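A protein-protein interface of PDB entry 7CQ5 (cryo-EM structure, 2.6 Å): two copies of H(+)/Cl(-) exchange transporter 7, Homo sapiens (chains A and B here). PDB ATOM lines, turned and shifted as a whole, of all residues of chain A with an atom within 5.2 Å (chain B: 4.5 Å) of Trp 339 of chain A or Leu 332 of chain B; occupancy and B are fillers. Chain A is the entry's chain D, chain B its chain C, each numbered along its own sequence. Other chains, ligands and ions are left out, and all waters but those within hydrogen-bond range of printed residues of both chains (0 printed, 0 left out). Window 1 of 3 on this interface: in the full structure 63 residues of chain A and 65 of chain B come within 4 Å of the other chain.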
ATOM      1  N   LEU A 332     -12.151  17.620  -9.208  1.00  0.00           N
ATOM      2  CA  LEU A 332     -11.798  17.857  -7.812  1.00  0.00           C
ATOM      3  C   LEU A 332     -10.372  18.360  -7.646  1.00  0.00           C
ATOM      4  O   LEU A 332     -10.082  19.053  -6.668  1.00  0.00           O
ATOM      5  CB  LEU A 332     -11.990  16.588  -6.989  1.00  0.00           C
ATOM      6  CG  LEU A 332     -13.435  16.163  -6.789  1.00  0.00           C
ATOM      7  CD1 LEU A 332     -13.507  14.845  -6.047  1.00  0.00           C
ATOM      8  CD2 LEU A 332     -14.202  17.251  -6.088  1.00  0.00           C
ATOM      9  N   SER A 337     -11.404  22.538  -3.566  1.00  0.00           N
ATOM     10  CA  SER A 337     -12.170  23.171  -2.512  1.00  0.00           C
ATOM     11  C   SER A 337     -12.258  22.279  -1.276  1.00  0.00           C
ATOM     12  O   SER A 337     -11.586  21.254  -1.164  1.00  0.00           O
ATOM     13  CB  SER A 337     -13.555  23.546  -3.038  1.00  0.00           C
ATOM     14  OG  SER A 337     -14.301  22.403  -3.396  1.00  0.00           O
ATOM     15  N   PHE A 338     -13.082  22.701  -0.322  1.00  0.00           N
ATOM     16  CA  PHE A 338     -13.522  21.846   0.766  1.00  0.00           C
ATOM     17  C   PHE A 338     -14.308  20.659   0.211  1.00  0.00           C
ATOM     18  O   PHE A 338     -14.820  20.691  -0.911  1.00  0.00           O
ATOM     19  CB  PHE A 338     -14.376  22.652   1.753  1.00  0.00           C
ATOM     20  CG  PHE A 338     -15.635  23.232   1.151  1.00  0.00           C
ATOM     21  CD1 PHE A 338     -15.618  24.477   0.529  1.00  0.00           C
ATOM     22  CD2 PHE A 338     -16.844  22.548   1.228  1.00  0.00           C
ATOM     23  CE1 PHE A 338     -16.767  25.005  -0.028  1.00  0.00           C
ATOM     24  CE2 PHE A 338     -17.990  23.072   0.671  1.00  0.00           C
ATOM     25  CZ  PHE A 338     -17.953  24.301   0.048  1.00  0.00           C
ATOM     26  N   TRP A 339     -14.424  19.608   1.012  1.00  0.00           N
ATOM     27  CA  TRP A 339     -15.186  18.451   0.567  1.00  0.00           C
ATOM     28  C   TRP A 339     -16.674  18.762   0.644  1.00  0.00           C
ATOM     29  O   TRP A 339     -17.194  19.088   1.714  1.00  0.00           O
ATOM     30  CB  TRP A 339     -14.864  17.205   1.382  1.00  0.00           C
ATOM     31  CG  TRP A 339     -15.591  16.014   0.865  1.00  0.00           C
ATOM     32  CD1 TRP A 339     -16.747  15.485   1.350  1.00  0.00           C
ATOM     33  CD2 TRP A 339     -15.223  15.210  -0.259  1.00  0.00           C
ATOM     34  NE1 TRP A 339     -17.120  14.402   0.602  1.00  0.00           N
ATOM     35  CE2 TRP A 339     -16.198  14.208  -0.389  1.00  0.00           C
ATOM     36  CE3 TRP A 339     -14.158  15.238  -1.164  1.00  0.00           C
ATOM     37  CZ2 TRP A 339     -16.142  13.246  -1.386  1.00  0.00           C
ATOM     38  CZ3 TRP A 339     -14.105  14.283  -2.148  1.00  0.00           C
ATOM     39  CH2 TRP A 339     -15.088  13.298  -2.250  1.00  0.00           C
ATOM     40  N   ASN A 340     -17.347  18.661  -0.493  1.00  0.00           N
ATOM     41  CA  ASN A 340     -18.778  18.901  -0.613  1.00  0.00           C
ATOM     42  C   ASN A 340     -19.381  17.606  -1.137  1.00  0.00           C
ATOM     43  O   ASN A 340     -19.198  17.266  -2.306  1.00  0.00           O
ATOM     44  CB  ASN A 340     -19.043  20.094  -1.536  1.00  0.00           C
ATOM     45  CG  ASN A 340     -20.493  20.558  -1.529  1.00  0.00           C
ATOM     46  OD1 ASN A 340     -21.367  19.934  -0.937  1.00  0.00           O
ATOM     47  ND2 ASN A 340     -20.742  21.691  -2.167  1.00  0.00           N
ATOM     48  N   GLN A 341     -20.087  16.889  -0.260  1.00  0.00           N
ATOM     49  CA  GLN A 341     -20.588  15.552  -0.576  1.00  0.00           C
ATOM     50  C   GLN A 341     -21.646  15.592  -1.672  1.00  0.00           C
ATOM     51  O   GLN A 341     -21.618  14.782  -2.611  1.00  0.00           O
ATOM     52  CB  GLN A 341     -21.154  14.920   0.699  1.00  0.00           C
ATOM     53  CG  GLN A 341     -21.627  13.488   0.602  1.00  0.00           C
ATOM     54  CD  GLN A 341     -20.508  12.524   0.322  1.00  0.00           C
ATOM     55  OE1 GLN A 341     -19.394  12.700   0.805  1.00  0.00           O
ATOM     56  NE2 GLN A 341     -20.802  11.481  -0.440  1.00  0.00           N
ATOM     57  N   THR A 344     -20.063  16.661  -5.187  1.00  0.00           N
ATOM     58  CA  THR A 344     -19.344  15.541  -5.789  1.00  0.00           C
ATOM     59  C   THR A 344     -20.292  14.456  -6.269  1.00  0.00           C
ATOM     60  O   THR A 344     -20.049  13.835  -7.312  1.00  0.00           O
ATOM     61  CB  THR A 344     -18.343  14.945  -4.801  1.00  0.00           C
ATOM     62  OG1 THR A 344     -19.004  14.641  -3.572  1.00  0.00           O
ATOM     63  CG2 THR A 344     -17.248  15.896  -4.532  1.00  0.00           C
ATOM     64  N   VAL B 328     -10.007   5.385  -1.662  1.00  0.00           N
ATOM     65  CA  VAL B 328      -9.688   6.805  -1.612  1.00  0.00           C
ATOM     66  C   VAL B 328     -10.955   7.630  -1.449  1.00  0.00           C
ATOM     67  O   VAL B 328     -11.005   8.556  -0.633  1.00  0.00           O
ATOM     68  CB  VAL B 328      -8.903   7.202  -2.874  1.00  0.00           C
ATOM     69  CG1 VAL B 328      -8.563   8.674  -2.868  1.00  0.00           C
ATOM     70  CG2 VAL B 328      -7.662   6.361  -2.994  1.00  0.00           C
ATOM     71  N   LEU B 329     -12.016   7.270  -2.172  1.00  0.00           N
ATOM     72  CA  LEU B 329     -13.274   7.987  -2.026  1.00  0.00           C
ATOM     73  C   LEU B 329     -13.963   7.676  -0.709  1.00  0.00           C
ATOM     74  O   LEU B 329     -14.731   8.502  -0.222  1.00  0.00           O
ATOM     75  CB  LEU B 329     -14.207   7.673  -3.187  1.00  0.00           C
ATOM     76  CG  LEU B 329     -13.766   8.233  -4.529  1.00  0.00           C
ATOM     77  CD1 LEU B 329     -14.740   7.791  -5.568  1.00  0.00           C
ATOM     78  CD2 LEU B 329     -13.678   9.737  -4.482  1.00  0.00           C
ATOM     79  N   PHE B 330     -13.723   6.503  -0.125  1.00  0.00           N
ATOM     80  CA  PHE B 330     -14.234   6.237   1.214  1.00  0.00           C
ATOM     81  C   PHE B 330     -13.566   7.138   2.238  1.00  0.00           C
ATOM     82  O   PHE B 330     -14.234   7.726   3.094  1.00  0.00           O
ATOM     83  CB  PHE B 330     -14.031   4.771   1.588  1.00  0.00           C
ATOM     84  CG  PHE B 330     -14.485   4.442   2.980  1.00  0.00           C
ATOM     85  CD1 PHE B 330     -15.831   4.354   3.274  1.00  0.00           C
ATOM     86  CD2 PHE B 330     -13.566   4.241   3.999  1.00  0.00           C
ATOM     87  CE1 PHE B 330     -16.254   4.067   4.555  1.00  0.00           C
ATOM     88  CE2 PHE B 330     -13.980   3.958   5.277  1.00  0.00           C
ATOM     89  CZ  PHE B 330     -15.325   3.867   5.556  1.00  0.00           C
ATOM     90  N   SER B 331     -12.249   7.261   2.165  1.00  0.00           N
ATOM     91  CA  SER B 331     -11.530   8.047   3.152  1.00  0.00           C
ATOM     92  C   SER B 331     -11.477   9.533   2.815  1.00  0.00           C
ATOM     93  O   SER B 331     -10.861  10.295   3.564  1.00  0.00           O
ATOM     94  CB  SER B 331     -10.118   7.494   3.322  1.00  0.00           C
ATOM     95  OG  SER B 331      -9.356   7.718   2.159  1.00  0.00           O
ATOM     96  N   LEU B 332     -12.074   9.961   1.701  1.00  0.00           N
ATOM     97  CA  LEU B 332     -12.327  11.377   1.461  1.00  0.00           C
ATOM     98  C   LEU B 332     -13.717  11.803   1.911  1.00  0.00           C
ATOM     99  O   LEU B 332     -13.903  12.954   2.317  1.00  0.00           O
ATOM    100  CB  LEU B 332     -12.154  11.723  -0.022  1.00  0.00           C
ATOM    101  CG  LEU B 332     -10.782  11.795  -0.694  1.00  0.00           C
ATOM    102  CD1 LEU B 332     -10.968  11.932  -2.187  1.00  0.00           C
ATOM    103  CD2 LEU B 332      -9.954  12.936  -0.161  1.00  0.00           C
ATOM    104  N   GLU B 333     -14.699  10.902   1.825  1.00  0.00           N
ATOM    105  CA  GLU B 333     -16.027  11.173   2.370  1.00  0.00           C
ATOM    106  C   GLU B 333     -15.986  11.325   3.882  1.00  0.00           C
ATOM    107  O   GLU B 333     -16.506  12.298   4.436  1.00  0.00           O
ATOM    108  CB  GLU B 333     -16.988  10.054   1.987  1.00  0.00           C
ATOM    109  CG  GLU B 333     -17.415  10.056   0.550  1.00  0.00           C
ATOM    110  CD  GLU B 333     -18.222   8.832   0.204  1.00  0.00           C
ATOM    111  OE1 GLU B 333     -18.299   7.914   1.046  1.00  0.00           O
ATOM    112  OE2 GLU B 333     -18.781   8.789  -0.905  1.00  0.00           O
ATOM    113  N   GLU B 334     -15.412  10.350   4.570  1.00  0.00           N
ATOM    114  CA  GLU B 334     -15.140  10.500   5.987  1.00  0.00           C
ATOM    115  C   GLU B 334     -13.834  11.259   6.143  1.00  0.00           C
ATOM    116  O   GLU B 334     -12.842  10.934   5.490  1.00  0.00           O
ATOM    117  CB  GLU B 334     -15.065   9.136   6.668  1.00  0.00           C
ATOM    118  CG  GLU B 334     -16.351   8.340   6.567  1.00  0.00           C
ATOM    119  CD  GLU B 334     -17.527   9.012   7.269  1.00  0.00           C
ATOM    120  OE1 GLU B 334     -17.318   9.702   8.294  1.00  0.00           O
ATOM    121  OE2 GLU B 334     -18.667   8.854   6.790  1.00  0.00           O
ATOM    122  N   GLY B 335     -13.823  12.268   6.997  1.00  0.00           N
ATOM    123  CA  GLY B 335     -12.706  13.184   6.941  1.00  0.00           C
ATOM    124  C   GLY B 335     -12.911  14.123   5.780  1.00  0.00           C
ATOM    125  O   GLY B 335     -12.147  14.127   4.814  1.00  0.00           O
ATOM    126  N   ALA B 336     -13.982  14.904   5.864  1.00  0.00           N
ATOM    127  CA  ALA B 336     -14.417  15.763   4.771  1.00  0.00           C
ATOM    128  C   ALA B 336     -13.708  17.105   4.908  1.00  0.00           C
ATOM    129  O   ALA B 336     -14.277  18.109   5.336  1.00  0.00           O
ATOM    130  CB  ALA B 336     -15.930  15.908   4.796  1.00  0.00           C
ATOM    131  N   SER B 337     -12.439  17.117   4.529  1.00  0.00           N
ATOM    132  CA  SER B 337     -11.597  18.282   4.713  1.00  0.00           C
ATOM    133  C   SER B 337     -11.415  19.034   3.400  1.00  0.00           C
ATOM    134  O   SER B 337     -12.020  18.718   2.376  1.00  0.00           O
ATOM    135  CB  SER B 337     -10.252  17.872   5.312  1.00  0.00           C
ATOM    136  OG  SER B 337      -9.515  17.051   4.432  1.00  0.00           O
ATOM    137  N   TRP B 339      -9.310  20.129   0.074  1.00  0.00           N
ATOM    138  CA  TRP B 339      -8.612  19.280  -0.885  1.00  0.00           C
ATOM    139  C   TRP B 339      -7.113  19.340  -0.637  1.00  0.00           C
ATOM    140  O   TRP B 339      -6.507  20.414  -0.684  1.00  0.00           O
ATOM    141  CB  TRP B 339      -8.922  19.690  -2.321  1.00  0.00           C
ATOM    142  CG  TRP B 339      -8.280  18.768  -3.311  1.00  0.00           C
ATOM    143  CD1 TRP B 339      -7.114  18.972  -3.981  1.00  0.00           C
ATOM    144  CD2 TRP B 339      -8.760  17.485  -3.726  1.00  0.00           C
ATOM    145  NE1 TRP B 339      -6.841  17.904  -4.793  1.00  0.00           N
ATOM    146  CE2 TRP B 339      -7.833  16.973  -4.650  1.00  0.00           C
ATOM    147  CE3 TRP B 339      -9.885  16.720  -3.405  1.00  0.00           C
ATOM    148  CZ2 TRP B 339      -8.000  15.738  -5.265  1.00  0.00           C
ATOM    149  CZ3 TRP B 339     -10.044  15.493  -4.013  1.00  0.00           C
ATOM    150  CH2 TRP B 339      -9.104  15.012  -4.929  1.00  0.00           C
ATOM    151  N   THR B 344      -3.972  12.991  -0.886  1.00  0.00           N
ATOM    152  CA  THR B 344      -4.823  12.106  -1.675  1.00  0.00           C
ATOM    153  C   THR B 344      -3.992  11.220  -2.592  1.00  0.00           C
ATOM    154  O   THR B 344      -4.321  10.045  -2.800  1.00  0.00           O
ATOM    155  CB  THR B 344      -5.818  12.947  -2.477  1.00  0.00           C
ATOM    156  OG1 THR B 344      -6.469  13.861  -1.595  1.00  0.00           O
ATOM    157  CG2 THR B 344      -6.889  12.083  -3.110  1.00  0.00           C
ATOM    158  N   LEU B 584     -21.531   6.900  -3.572  1.00  0.00           N
ATOM    159  CA  LEU B 584     -20.339   7.492  -4.192  1.00  0.00           C
ATOM    160  C   LEU B 584     -19.035   6.794  -3.829  1.00  0.00           C
ATOM    161  O   LEU B 584     -18.071   6.831  -4.598  1.00  0.00           O
ATOM    162  CB  LEU B 584     -20.235   8.985  -3.838  1.00  0.00           C
ATOM    163  CG  LEU B 584     -19.115   9.878  -4.372  1.00  0.00           C
ATOM    164  CD1 LEU B 584     -19.160   9.903  -5.880  1.00  0.00           C
ATOM    165  CD2 LEU B 584     -19.230  11.277  -3.799  1.00  0.00           C
ATOM    166  N   TRP B 636     -22.320  16.057   7.272  1.00  0.00           N
ATOM    167  CA  TRP B 636     -21.619  16.819   6.247  1.00  0.00           C
ATOM    168  C   TRP B 636     -21.990  18.295   6.246  1.00  0.00           C
ATOM    169  O   TRP B 636     -21.165  19.125   5.857  1.00  0.00           O
ATOM    170  CB  TRP B 636     -21.860  16.241   4.857  1.00  0.00           C
ATOM    171  CG  TRP B 636     -21.175  14.947   4.599  1.00  0.00           C
ATOM    172  CD1 TRP B 636     -19.835  14.753   4.433  1.00  0.00           C
ATOM    173  CD2 TRP B 636     -21.797  13.685   4.346  1.00  0.00           C
ATOM    174  NE1 TRP B 636     -19.580  13.435   4.159  1.00  0.00           N
ATOM    175  CE2 TRP B 636     -20.769  12.758   4.091  1.00  0.00           C
ATOM    176  CE3 TRP B 636     -23.122  13.243   4.332  1.00  0.00           C
ATOM    177  CZ2 TRP B 636     -21.024  11.418   3.830  1.00  0.00           C
ATOM    178  CZ3 TRP B 636     -23.373  11.914   4.076  1.00  0.00           C
ATOM    179  CH2 TRP B 636     -22.331  11.016   3.829  1.00  0.00           C
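The indole nitrogen (NE1) of Trp 636 of chain B sits at hydrogen-bond distance from the backbone carbonyl oxygen (O) of Glu 333 of chain B, at 3.3 Å. The indole nitrogen (NE1) of Trp 339 of chain A sits at hydrogen-bond distance from the side-chain amide oxygen (OE1) of Gln 341 of chain A, at 2.8 Å. The backbone carbonyl oxygen (O) of Asn 340 of chain A lies within hydrogen-bond range of the side-chain hydroxyl (OG1) of Thr 344 of chain A (2.9 Å). OG1 of Thr 344 of chain A sits at hydrogen-bond distance from O of Gln 341 of chain A (2.8 Å).
CD2 of Trp 339 of chain B touches O of Leu 332 of chain A, at 3.6 Å. C of Phe 338 of chain A touches O of Ser 337 of chain B, at 3.7 Å. Trp 339 of chain A touches Leu 332 of chain B (CD2 to O, 3.7 Å). CA of Glu 333 of chain B touches NE1 of Trp 339 of chain A, at 3.8 Å. CB of Ala 336 of chain B touches CD1 of Trp 339 of chain A, at 3.6 Å. Gln 341 of chain A touches Leu 584 of chain B (NE2 to CD2, 3.7 Å). OG1 of Thr 344 of chain A touches CD2 of Leu 584 of chain B, 3.4 Å away.
Of the printed residues of chain B, Leu 332 of chain A touches Trp 339 (3.6 Å). Of the printed residues of chain B, Gln 341 of chain A touches Glu 333, Leu 584 and Trp 636. Leu 329 of chain B touches none of the printed residues of chain A. Leu 332 of chain B touches just one residue of chain A: Trp 339. Of the printed residues of chain A, Trp 339 of chain B touches Leu 332 and Ser 337. Of the printed residues of chain A, Leu 584 of chain B touches Gln 341 and Thr 344. Printed residues of chain A within 4 Å of Trp 636 of chain B: Gln 341. The nearest printed residue of chain A that does not touch Leu 332 of chain B is Leu 332 of chain A (5.5 Å). The nearest printed residue of chain A that does not touch Ala 336 of chain B is Phe 338 of chain A (5.7 Å).
Leu 332 of chain A touches Trp 339 of chain B, and with the chains exchanged Trp 339 of chain A touches Leu 332 of chain B. Ser 337 of chain A touches Trp 339 of chain B, and with the chains exchanged Trp 339 of chain A touches Ser 337 of chain B. Positions printed for both chains: 332, 337, 339 and 344. Of the 11 pairs that touch across the chains among the printed residues, 4 have their exchanged pair printed and touching as well.
OE2 of Glu 333 of chain B sits at hydrogen-bond distance from NE2 of Gln 341 of chain A (3.4 Å). The backbone NH of Trp 339 of chain A sits at hydrogen-bond distance from the backbone carbonyl oxygen of Ser 337 of chain B (2.9 Å). The backbone NH of Trp 339 of chain B sits at hydrogen-bond distance from the backbone carbonyl oxygen of Ser 337 of chain A, at 2.8 Å. The indole nitrogen of Trp 636 of chain B sits at hydrogen-bond distance from the side-chain amide oxygen of Gln 341 of chain A (3.4 Å).
Of the 7 printed residues of chain A, 6 touch a printed residue of chain B. Hydrophobic or aromatic side chains of chain A that line the printed part of chain B: Leu 332 and Trp 339. Along chain A the printed residues that touch a printed residue of chain B span positions 332 to 344. Of the 14 printed residues of chain B, 7 touch a printed residue of chain A. Hydrophobic or aromatic side chains of chain B that line the printed part of chain A: Leu 332, Ala 336, Trp 339, Leu 584 and Trp 636. Along chain B the printed residues that touch a printed residue of chain A span positions 332 to 636. Among the printed residues, 11 pairs touch across the chains. Among the printed residues, no Asp or Glu carboxylate lies within 4 Å of a Lys or Arg side-chain nitrogen of the other chain.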
